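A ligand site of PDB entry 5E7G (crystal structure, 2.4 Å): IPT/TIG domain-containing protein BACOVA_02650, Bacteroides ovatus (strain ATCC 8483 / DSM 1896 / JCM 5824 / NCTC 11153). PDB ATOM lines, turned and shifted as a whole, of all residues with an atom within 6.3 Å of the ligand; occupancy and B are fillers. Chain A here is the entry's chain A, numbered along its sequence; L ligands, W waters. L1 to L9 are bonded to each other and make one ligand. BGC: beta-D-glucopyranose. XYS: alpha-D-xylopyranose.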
ATOM      1  N   VAL A 296     -34.092 -11.760 -18.423  1.00  0.00           N
ATOM      2  CA  VAL A 296     -32.773 -11.169 -18.231  1.00  0.00           C
ATOM      3  C   VAL A 296     -31.769 -11.752 -19.234  1.00  0.00           C
ATOM      4  O   VAL A 296     -31.152 -11.011 -19.990  1.00  0.00           O
ATOM      5  CB  VAL A 296     -32.237 -11.384 -16.801  1.00  0.00           C
ATOM      6  CG1 VAL A 296     -30.857 -10.772 -16.657  1.00  0.00           C
ATOM      7  CG2 VAL A 296     -33.196 -10.783 -15.769  1.00  0.00           C
ATOM      8  N   TRP A 297     -31.610 -13.065 -19.212  1.00  0.00           N
ATOM      9  CA  TRP A 297     -30.640 -13.733 -20.073  1.00  0.00           C
ATOM     10  C   TRP A 297     -31.051 -15.178 -20.327  1.00  0.00           C
ATOM     11  O   TRP A 297     -31.948 -15.701 -19.675  1.00  0.00           O
ATOM     12  CB  TRP A 297     -29.245 -13.694 -19.428  1.00  0.00           C
ATOM     13  CG  TRP A 297     -29.150 -14.436 -18.115  1.00  0.00           C
ATOM     14  CD1 TRP A 297     -29.355 -13.931 -16.853  1.00  0.00           C
ATOM     15  CD2 TRP A 297     -28.812 -15.824 -17.927  1.00  0.00           C
ATOM     16  NE1 TRP A 297     -29.173 -14.911 -15.913  1.00  0.00           N
ATOM     17  CE2 TRP A 297     -28.844 -16.079 -16.536  1.00  0.00           C
ATOM     18  CE3 TRP A 297     -28.505 -16.872 -18.804  1.00  0.00           C
ATOM     19  CZ2 TRP A 297     -28.571 -17.336 -16.007  1.00  0.00           C
ATOM     20  CZ3 TRP A 297     -28.234 -18.116 -18.270  1.00  0.00           C
ATOM     21  CH2 TRP A 297     -28.267 -18.336 -16.891  1.00  0.00           C
ATOM     22  N   GLY A 298     -30.372 -15.809 -21.285  1.00  0.00           N
ATOM     23  CA  GLY A 298     -30.583 -17.213 -21.581  1.00  0.00           C
ATOM     24  C   GLY A 298     -30.741 -17.473 -23.071  1.00  0.00           C
ATOM     25  O   GLY A 298     -31.159 -16.596 -23.830  1.00  0.00           O
ATOM     26  N   TYR A 330     -27.237 -31.617 -20.640  1.00  0.00           N
ATOM     27  CA  TYR A 330     -27.692 -31.159 -19.326  1.00  0.00           C
ATOM     28  C   TYR A 330     -27.600 -29.636 -19.188  1.00  0.00           C
ATOM     29  O   TYR A 330     -27.787 -29.094 -18.088  1.00  0.00           O
ATOM     30  CB  TYR A 330     -26.887 -31.852 -18.227  1.00  0.00           C
ATOM     31  CG  TYR A 330     -27.099 -33.350 -18.226  1.00  0.00           C
ATOM     32  CD1 TYR A 330     -28.191 -33.917 -17.583  1.00  0.00           C
ATOM     33  CD2 TYR A 330     -26.216 -34.199 -18.878  1.00  0.00           C
ATOM     34  CE1 TYR A 330     -28.393 -35.293 -17.595  1.00  0.00           C
ATOM     35  CE2 TYR A 330     -26.405 -35.570 -18.896  1.00  0.00           C
ATOM     36  CZ  TYR A 330     -27.506 -36.109 -18.251  1.00  0.00           C
ATOM     37  OH  TYR A 330     -27.710 -37.471 -18.258  1.00  0.00           O
ATOM     38  N   TRP A 331     -27.327 -28.955 -20.289  1.00  0.00           N
ATOM     39  CA  TRP A 331     -27.435 -27.508 -20.354  1.00  0.00           C
ATOM     40  C   TRP A 331     -27.661 -27.025 -21.787  1.00  0.00           C
ATOM     41  O   TRP A 331     -26.704 -26.738 -22.518  1.00  0.00           O
ATOM     42  CB  TRP A 331     -26.192 -26.838 -19.773  1.00  0.00           C
ATOM     43  CG  TRP A 331     -26.279 -25.346 -19.788  1.00  0.00           C
ATOM     44  CD1 TRP A 331     -25.691 -24.495 -20.681  1.00  0.00           C
ATOM     45  CD2 TRP A 331     -27.003 -24.524 -18.864  1.00  0.00           C
ATOM     46  NE1 TRP A 331     -26.007 -23.192 -20.371  1.00  0.00           N
ATOM     47  CE2 TRP A 331     -26.807 -23.179 -19.265  1.00  0.00           C
ATOM     48  CE3 TRP A 331     -27.795 -24.785 -17.742  1.00  0.00           C
ATOM     49  CZ2 TRP A 331     -27.379 -22.109 -18.573  1.00  0.00           C
ATOM     50  CZ3 TRP A 331     -28.357 -23.721 -17.069  1.00  0.00           C
ATOM     51  CH2 TRP A 331     -28.150 -22.406 -17.485  1.00  0.00           C
ATOM     52  N   GLN A 334     -32.725 -22.157 -22.142  1.00  0.00           N
ATOM     53  CA  GLN A 334     -33.350 -21.736 -20.904  1.00  0.00           C
ATOM     54  C   GLN A 334     -33.650 -20.243 -20.893  1.00  0.00           C
ATOM     55  O   GLN A 334     -33.137 -19.498 -21.723  1.00  0.00           O
ATOM     56  CB  GLN A 334     -32.432 -22.100 -19.714  1.00  0.00           C
ATOM     57  CG  GLN A 334     -31.097 -21.332 -19.673  1.00  0.00           C
ATOM     58  CD  GLN A 334     -30.143 -21.731 -20.791  1.00  0.00           C
ATOM     59  OE1 GLN A 334     -29.635 -20.878 -21.526  1.00  0.00           O
ATOM     60  NE2 GLN A 334     -29.897 -23.027 -20.912  1.00  0.00           N
ATOM     61  N   TYR A 336     -33.777 -17.172 -17.895  1.00  0.00           N
ATOM     62  CA  TYR A 336     -33.613 -16.669 -16.530  1.00  0.00           C
ATOM     63  C   TYR A 336     -34.285 -15.313 -16.466  1.00  0.00           C
ATOM     64  O   TYR A 336     -33.824 -14.362 -17.101  1.00  0.00           O
ATOM     65  CB  TYR A 336     -32.125 -16.568 -16.158  1.00  0.00           C
ATOM     66  CG  TYR A 336     -31.837 -16.153 -14.732  1.00  0.00           C
ATOM     67  CD1 TYR A 336     -32.202 -14.904 -14.252  1.00  0.00           C
ATOM     68  CD2 TYR A 336     -31.186 -17.020 -13.843  1.00  0.00           C
ATOM     69  CE1 TYR A 336     -31.942 -14.517 -12.960  1.00  0.00           C
ATOM     70  CE2 TYR A 336     -30.918 -16.639 -12.534  1.00  0.00           C
ATOM     71  CZ  TYR A 336     -31.314 -15.382 -12.105  1.00  0.00           C
ATOM     72  OH  TYR A 336     -31.068 -14.975 -10.812  1.00  0.00           O
ATOM     73  N   GLN A 374     -36.988 -27.796 -16.126  1.00  0.00           N
ATOM     74  CA  GLN A 374     -36.814 -27.428 -14.727  1.00  0.00           C
ATOM     75  C   GLN A 374     -37.379 -26.033 -14.484  1.00  0.00           C
ATOM     76  O   GLN A 374     -37.102 -25.109 -15.243  1.00  0.00           O
ATOM     77  CB  GLN A 374     -35.342 -27.469 -14.333  1.00  0.00           C
ATOM     78  CG  GLN A 374     -35.059 -26.992 -12.909  1.00  0.00           C
ATOM     79  CD  GLN A 374     -33.576 -26.911 -12.586  1.00  0.00           C
ATOM     80  OE1 GLN A 374     -32.744 -26.723 -13.471  1.00  0.00           O
ATOM     81  NE2 GLN A 374     -33.239 -27.052 -11.312  1.00  0.00           N
ATOM     82  N   GLU A 379     -33.372 -18.648  -6.720  1.00  0.00           N
ATOM     83  CA  GLU A 379     -32.045 -19.255  -6.708  1.00  0.00           C
ATOM     84  C   GLU A 379     -31.971 -20.486  -5.803  1.00  0.00           C
ATOM     85  O   GLU A 379     -30.883 -21.008  -5.562  1.00  0.00           O
ATOM     86  CB  GLU A 379     -30.993 -18.223  -6.267  1.00  0.00           C
ATOM     87  CG  GLU A 379     -30.794 -17.076  -7.255  1.00  0.00           C
ATOM     88  CD  GLU A 379     -29.742 -17.371  -8.321  1.00  0.00           C
ATOM     89  OE1 GLU A 379     -29.013 -18.376  -8.176  1.00  0.00           O
ATOM     90  OE2 GLU A 379     -29.634 -16.590  -9.295  1.00  0.00           O
ATOM     91  N   PHE A 381     -32.231 -23.813  -6.080  1.00  0.00           N
ATOM     92  CA  PHE A 381     -32.304 -24.935  -7.009  1.00  0.00           C
ATOM     93  C   PHE A 381     -32.516 -26.272  -6.306  1.00  0.00           C
ATOM     94  O   PHE A 381     -32.962 -27.239  -6.928  1.00  0.00           O
ATOM     95  CB  PHE A 381     -31.030 -24.957  -7.857  1.00  0.00           C
ATOM     96  CG  PHE A 381     -30.876 -23.736  -8.718  1.00  0.00           C
ATOM     97  CD1 PHE A 381     -31.536 -23.634  -9.934  1.00  0.00           C
ATOM     98  CD2 PHE A 381     -30.089 -22.672  -8.296  1.00  0.00           C
ATOM     99  CE1 PHE A 381     -31.409 -22.502 -10.739  1.00  0.00           C
ATOM    100  CE2 PHE A 381     -29.949 -21.537  -9.083  1.00  0.00           C
ATOM    101  CZ  PHE A 381     -30.616 -21.453 -10.313  1.00  0.00           C
ATOM    102  N   ASN A 386     -38.094 -30.457 -11.093  1.00  0.00           N
ATOM    103  CA  ASN A 386     -37.218 -31.078 -12.089  1.00  0.00           C
ATOM    104  C   ASN A 386     -37.890 -32.188 -12.875  1.00  0.00           C
ATOM    105  O   ASN A 386     -38.866 -32.802 -12.433  1.00  0.00           O
ATOM    106  CB  ASN A 386     -35.962 -31.634 -11.420  1.00  0.00           C
ATOM    107  CG  ASN A 386     -34.930 -30.553 -11.129  1.00  0.00           C
ATOM    108  OD1 ASN A 386     -34.353 -29.975 -12.055  1.00  0.00           O
ATOM    109  ND2 ASN A 386     -34.705 -30.274  -9.853  1.00  0.00           N
ATOM    110  N   TYR A 433     -35.675 -24.071 -17.479  1.00  0.00           N
ATOM    111  CA  TYR A 433     -34.482 -24.676 -18.073  1.00  0.00           C
ATOM    112  C   TYR A 433     -34.869 -25.947 -18.796  1.00  0.00           C
ATOM    113  O   TYR A 433     -35.481 -26.830 -18.204  1.00  0.00           O
ATOM    114  CB  TYR A 433     -33.428 -24.982 -16.992  1.00  0.00           C
ATOM    115  CG  TYR A 433     -33.087 -23.800 -16.121  1.00  0.00           C
ATOM    116  CD1 TYR A 433     -33.878 -23.476 -15.016  1.00  0.00           C
ATOM    117  CD2 TYR A 433     -31.983 -23.007 -16.374  1.00  0.00           C
ATOM    118  CE1 TYR A 433     -33.576 -22.400 -14.205  1.00  0.00           C
ATOM    119  CE2 TYR A 433     -31.662 -21.918 -15.569  1.00  0.00           C
ATOM    120  CZ  TYR A 433     -32.470 -21.620 -14.486  1.00  0.00           C
ATOM    121  OH  TYR A 433     -32.168 -20.543 -13.676  1.00  0.00           O
HETATM  122  C2  BGC L   1     -27.458  -8.046 -17.875  1.00  0.00           C
HETATM  123  C3  BGC L   1     -26.518  -9.191 -17.893  1.00  0.00           C
HETATM  124  C4  BGC L   1     -26.724 -10.079 -19.042  1.00  0.00           C
HETATM  125  C5  BGC L   1     -26.816  -9.350 -20.339  1.00  0.00           C
HETATM  126  C6  BGC L   1     -27.205 -10.350 -21.419  1.00  0.00           C
HETATM  127  C1  BGC L   1     -27.429  -7.228 -19.193  1.00  0.00           C
HETATM  128  O1  BGC L   1     -28.269  -6.238 -19.170  1.00  0.00           O
HETATM  129  O2  BGC L   1     -27.111  -7.174 -16.802  1.00  0.00           O
HETATM  130  O3  BGC L   1     -26.693  -9.979 -16.654  1.00  0.00           O
HETATM  131  O4  BGC L   1     -25.583 -10.993 -19.147  1.00  0.00           O
HETATM  132  O5  BGC L   1     -27.788  -8.245 -20.294  1.00  0.00           O
HETATM  133  O6  BGC L   1     -27.395  -9.679 -22.649  1.00  0.00           O
HETATM  134  C2  BGC L   2     -24.915 -13.354 -18.987  1.00  0.00           C
HETATM  135  C3  BGC L   2     -25.121 -14.624 -18.256  1.00  0.00           C
HETATM  136  C4  BGC L   2     -24.900 -14.496 -16.815  1.00  0.00           C
HETATM  137  C5  BGC L   2     -25.708 -13.376 -16.233  1.00  0.00           C
HETATM  138  C6  BGC L   2     -25.238 -13.082 -14.832  1.00  0.00           C
HETATM  139  C1  BGC L   2     -25.815 -12.224 -18.448  1.00  0.00           C
HETATM  140  O2  BGC L   2     -25.227 -13.545 -20.367  1.00  0.00           O
HETATM  141  O3  BGC L   2     -24.180 -15.627 -18.788  1.00  0.00           O
HETATM  142  O4  BGC L   2     -25.322 -15.728 -16.114  1.00  0.00           O
HETATM  143  O5  BGC L   2     -25.615 -12.095 -16.939  1.00  0.00           O
HETATM  144  O6  BGC L   2     -25.634 -14.109 -13.940  1.00  0.00           O
HETATM  145  C2  BGC L   3     -24.811 -17.985 -15.272  1.00  0.00           C
HETATM  146  C3  BGC L   3     -24.219 -19.327 -15.501  1.00  0.00           C
HETATM  147  C4  BGC L   3     -24.219 -19.765 -16.882  1.00  0.00           C
HETATM  148  C5  BGC L   3     -23.711 -18.701 -17.784  1.00  0.00           C
HETATM  149  C6  BGC L   3     -23.763 -19.155 -19.225  1.00  0.00           C
HETATM  150  C1  BGC L   3     -24.458 -16.873 -16.279  1.00  0.00           C
HETATM  151  O2  BGC L   3     -24.370 -17.557 -13.990  1.00  0.00           O
HETATM  152  O3  BGC L   3     -24.994 -20.322 -14.733  1.00  0.00           O
HETATM  153  O4  BGC L   3     -23.326 -20.939 -17.001  1.00  0.00           O
HETATM  154  O5  BGC L   3     -24.459 -17.440 -17.688  1.00  0.00           O
HETATM  155  O6  BGC L   3     -22.514 -19.737 -19.503  1.00  0.00           O
HETATM  156  C1  XYS L   4     -25.715 -13.645 -12.580  1.00  0.00           C
HETATM  157  C2  XYS L   4     -24.376 -13.829 -11.860  1.00  0.00           C
HETATM  158  C3  XYS L   4     -24.097 -15.264 -11.599  1.00  0.00           C
HETATM  159  C4  XYS L   4     -25.192 -15.866 -10.791  1.00  0.00           C
HETATM  160  C5  XYS L   4     -26.549 -15.717 -11.466  1.00  0.00           C
HETATM  161  O2  XYS L   4     -23.278 -13.288 -12.630  1.00  0.00           O
HETATM  162  O3  XYS L   4     -22.831 -15.392 -10.895  1.00  0.00           O
HETATM  163  O4  XYS L   4     -24.930 -17.266 -10.604  1.00  0.00           O
HETATM  164  O5  XYS L   4     -26.843 -14.332 -11.863  1.00  0.00           O
HETATM  165  C2  BGC L   5     -23.090 -23.411 -16.995  1.00  0.00           C
HETATM  166  C3  BGC L   5     -23.753 -24.718 -16.694  1.00  0.00           C
HETATM  167  C4  BGC L   5     -24.289 -24.796 -15.343  1.00  0.00           C
HETATM  168  C5  BGC L   5     -25.042 -23.568 -14.952  1.00  0.00           C
HETATM  169  C6  BGC L   5     -25.335 -23.607 -13.478  1.00  0.00           C
HETATM  170  C1  BGC L   5     -23.966 -22.178 -16.668  1.00  0.00           C
HETATM  171  O2  BGC L   5     -22.748 -23.356 -18.371  1.00  0.00           O
HETATM  172  O3  BGC L   5     -22.824 -25.843 -16.863  1.00  0.00           O
HETATM  173  O4  BGC L   5     -25.259 -25.915 -15.294  1.00  0.00           O
HETATM  174  O5  BGC L   5     -24.368 -22.291 -15.209  1.00  0.00           O
HETATM  175  O6  BGC L   5     -26.652 -24.083 -13.356  1.00  0.00           O
HETATM  176  C1  XYS L   6     -22.057 -19.576 -20.846  1.00  0.00           C
HETATM  177  C2  XYS L   6     -22.128 -20.898 -21.559  1.00  0.00           C
HETATM  178  C3  XYS L   6     -21.339 -21.884 -20.777  1.00  0.00           C
HETATM  179  C4  XYS L   6     -19.926 -21.456 -20.602  1.00  0.00           C
HETATM  180  C5  XYS L   6     -19.776 -19.993 -20.152  1.00  0.00           C
HETATM  181  O2  XYS L   6     -23.500 -21.351 -21.693  1.00  0.00           O
HETATM  182  O3  XYS L   6     -21.392 -23.183 -21.445  1.00  0.00           O
HETATM  183  O4  XYS L   6     -19.308 -22.304 -19.619  1.00  0.00           O
HETATM  184  O5  XYS L   6     -20.670 -19.061 -20.863  1.00  0.00           O
HETATM  185  C2  BGC L   7     -25.812 -28.180 -14.569  1.00  0.00           C
HETATM  186  C3  BGC L   7     -25.310 -29.528 -14.218  1.00  0.00           C
HETATM  187  C4  BGC L   7     -24.562 -30.129 -15.319  1.00  0.00           C
HETATM  188  C5  BGC L   7     -23.479 -29.229 -15.795  1.00  0.00           C
HETATM  189  C6  BGC L   7     -22.825 -29.879 -16.991  1.00  0.00           C
HETATM  190  C1  BGC L   7     -24.700 -27.203 -15.012  1.00  0.00           C
HETATM  191  O2  BGC L   7     -26.480 -27.650 -13.426  1.00  0.00           O
HETATM  192  O3  BGC L   7     -26.440 -30.410 -13.864  1.00  0.00           O
HETATM  193  O4  BGC L   7     -23.938 -31.388 -14.851  1.00  0.00           O
HETATM  194  O5  BGC L   7     -23.916 -27.862 -16.149  1.00  0.00           O
HETATM  195  O6  BGC L   7     -22.952 -29.001 -18.095  1.00  0.00           O
HETATM  196  C1  XYS L   8     -27.457 -23.364 -12.400  1.00  0.00           C
HETATM  197  C2  XYS L   8     -27.646 -24.225 -11.177  1.00  0.00           C
HETATM  198  C3  XYS L   8     -28.311 -25.493 -11.561  1.00  0.00           C
HETATM  199  C4  XYS L   8     -29.506 -25.324 -12.451  1.00  0.00           C
HETATM  200  C5  XYS L   8     -29.416 -24.217 -13.501  1.00  0.00           C
HETATM  201  O2  XYS L   8     -26.355 -24.497 -10.588  1.00  0.00           O
HETATM  202  O3  XYS L   8     -28.753 -26.189 -10.357  1.00  0.00           O
HETATM  203  O4  XYS L   8     -29.734 -26.564 -13.129  1.00  0.00           O
HETATM  204  O5  XYS L   8     -28.737 -22.993 -13.021  1.00  0.00           O
HETATM  205  C2  BGC L   9     -23.793 -33.780 -15.182  1.00  0.00           C
HETATM  206  C3  BGC L   9     -24.510 -35.075 -15.303  1.00  0.00           C
HETATM  207  C4  BGC L   9     -25.476 -35.277 -14.227  1.00  0.00           C
HETATM  208  C5  BGC L   9     -26.477 -34.166 -14.189  1.00  0.00           C
HETATM  209  C6  BGC L   9     -27.451 -34.375 -13.041  1.00  0.00           C
HETATM  210  C1  BGC L   9     -24.731 -32.567 -15.085  1.00  0.00           C
HETATM  211  O2  BGC L   9     -22.961 -33.590 -16.322  1.00  0.00           O
HETATM  212  O3  BGC L   9     -23.539 -36.180 -15.290  1.00  0.00           O
HETATM  213  O4  BGC L   9     -26.142 -36.580 -14.424  1.00  0.00           O
HETATM  214  O5  BGC L   9     -25.853 -32.838 -14.056  1.00  0.00           O
HETATM  215  O6  BGC L   9     -28.774 -34.295 -13.510  1.00  0.00           O
HETATM  216  O   HOH W   1     -29.370 -20.359 -13.742  1.00  0.00           O
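An oxygen (O4) of XYS L8 is in hydrogen-bond range of the side-chain amide oxygen (OE1) of Gln 374 (3.0 Å). An oxygen (O2) of XYS L6 is in hydrogen-bond range of the indole nitrogen of Trp 331 (3.4 Å).
N of Gln 374 lies within hydrogen-bond range of O of Tyr 433, 2.7 Å away. O of Trp 297 sits at hydrogen-bond distance from N of Tyr 336. The side-chain amide nitrogen (NE2) of Gln 374 lies close to the side-chain amide oxygen (OD1) of Asn 386, 3.2 Å away. The side-chain carboxylate (OE2) of Glu 379 lies within hydrogen-bond range of the side-chain hydroxyl (OH) of Tyr 336 (2.6 Å).
CE2 of Trp 297 touches O4 of BGC L2 (3.6 Å). CD1 of Tyr 330 touches C5 of BGC L9, 3.8 Å away. OE2 of Glu 379 touches C5 of XYS L4, at 3.9 Å. CE1 of Phe 381 touches O5 of XYS L8, 3.5 Å away. CE2 of Tyr 433 touches C5 of XYS L8, 3.8 Å away. Along chain A the residues within 4 Å of the ligand span positions 297 to 433.
Water W1 bridges O5 of XYS L8 (2.8 Å) and OH of Tyr 433 (2.8 Å).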
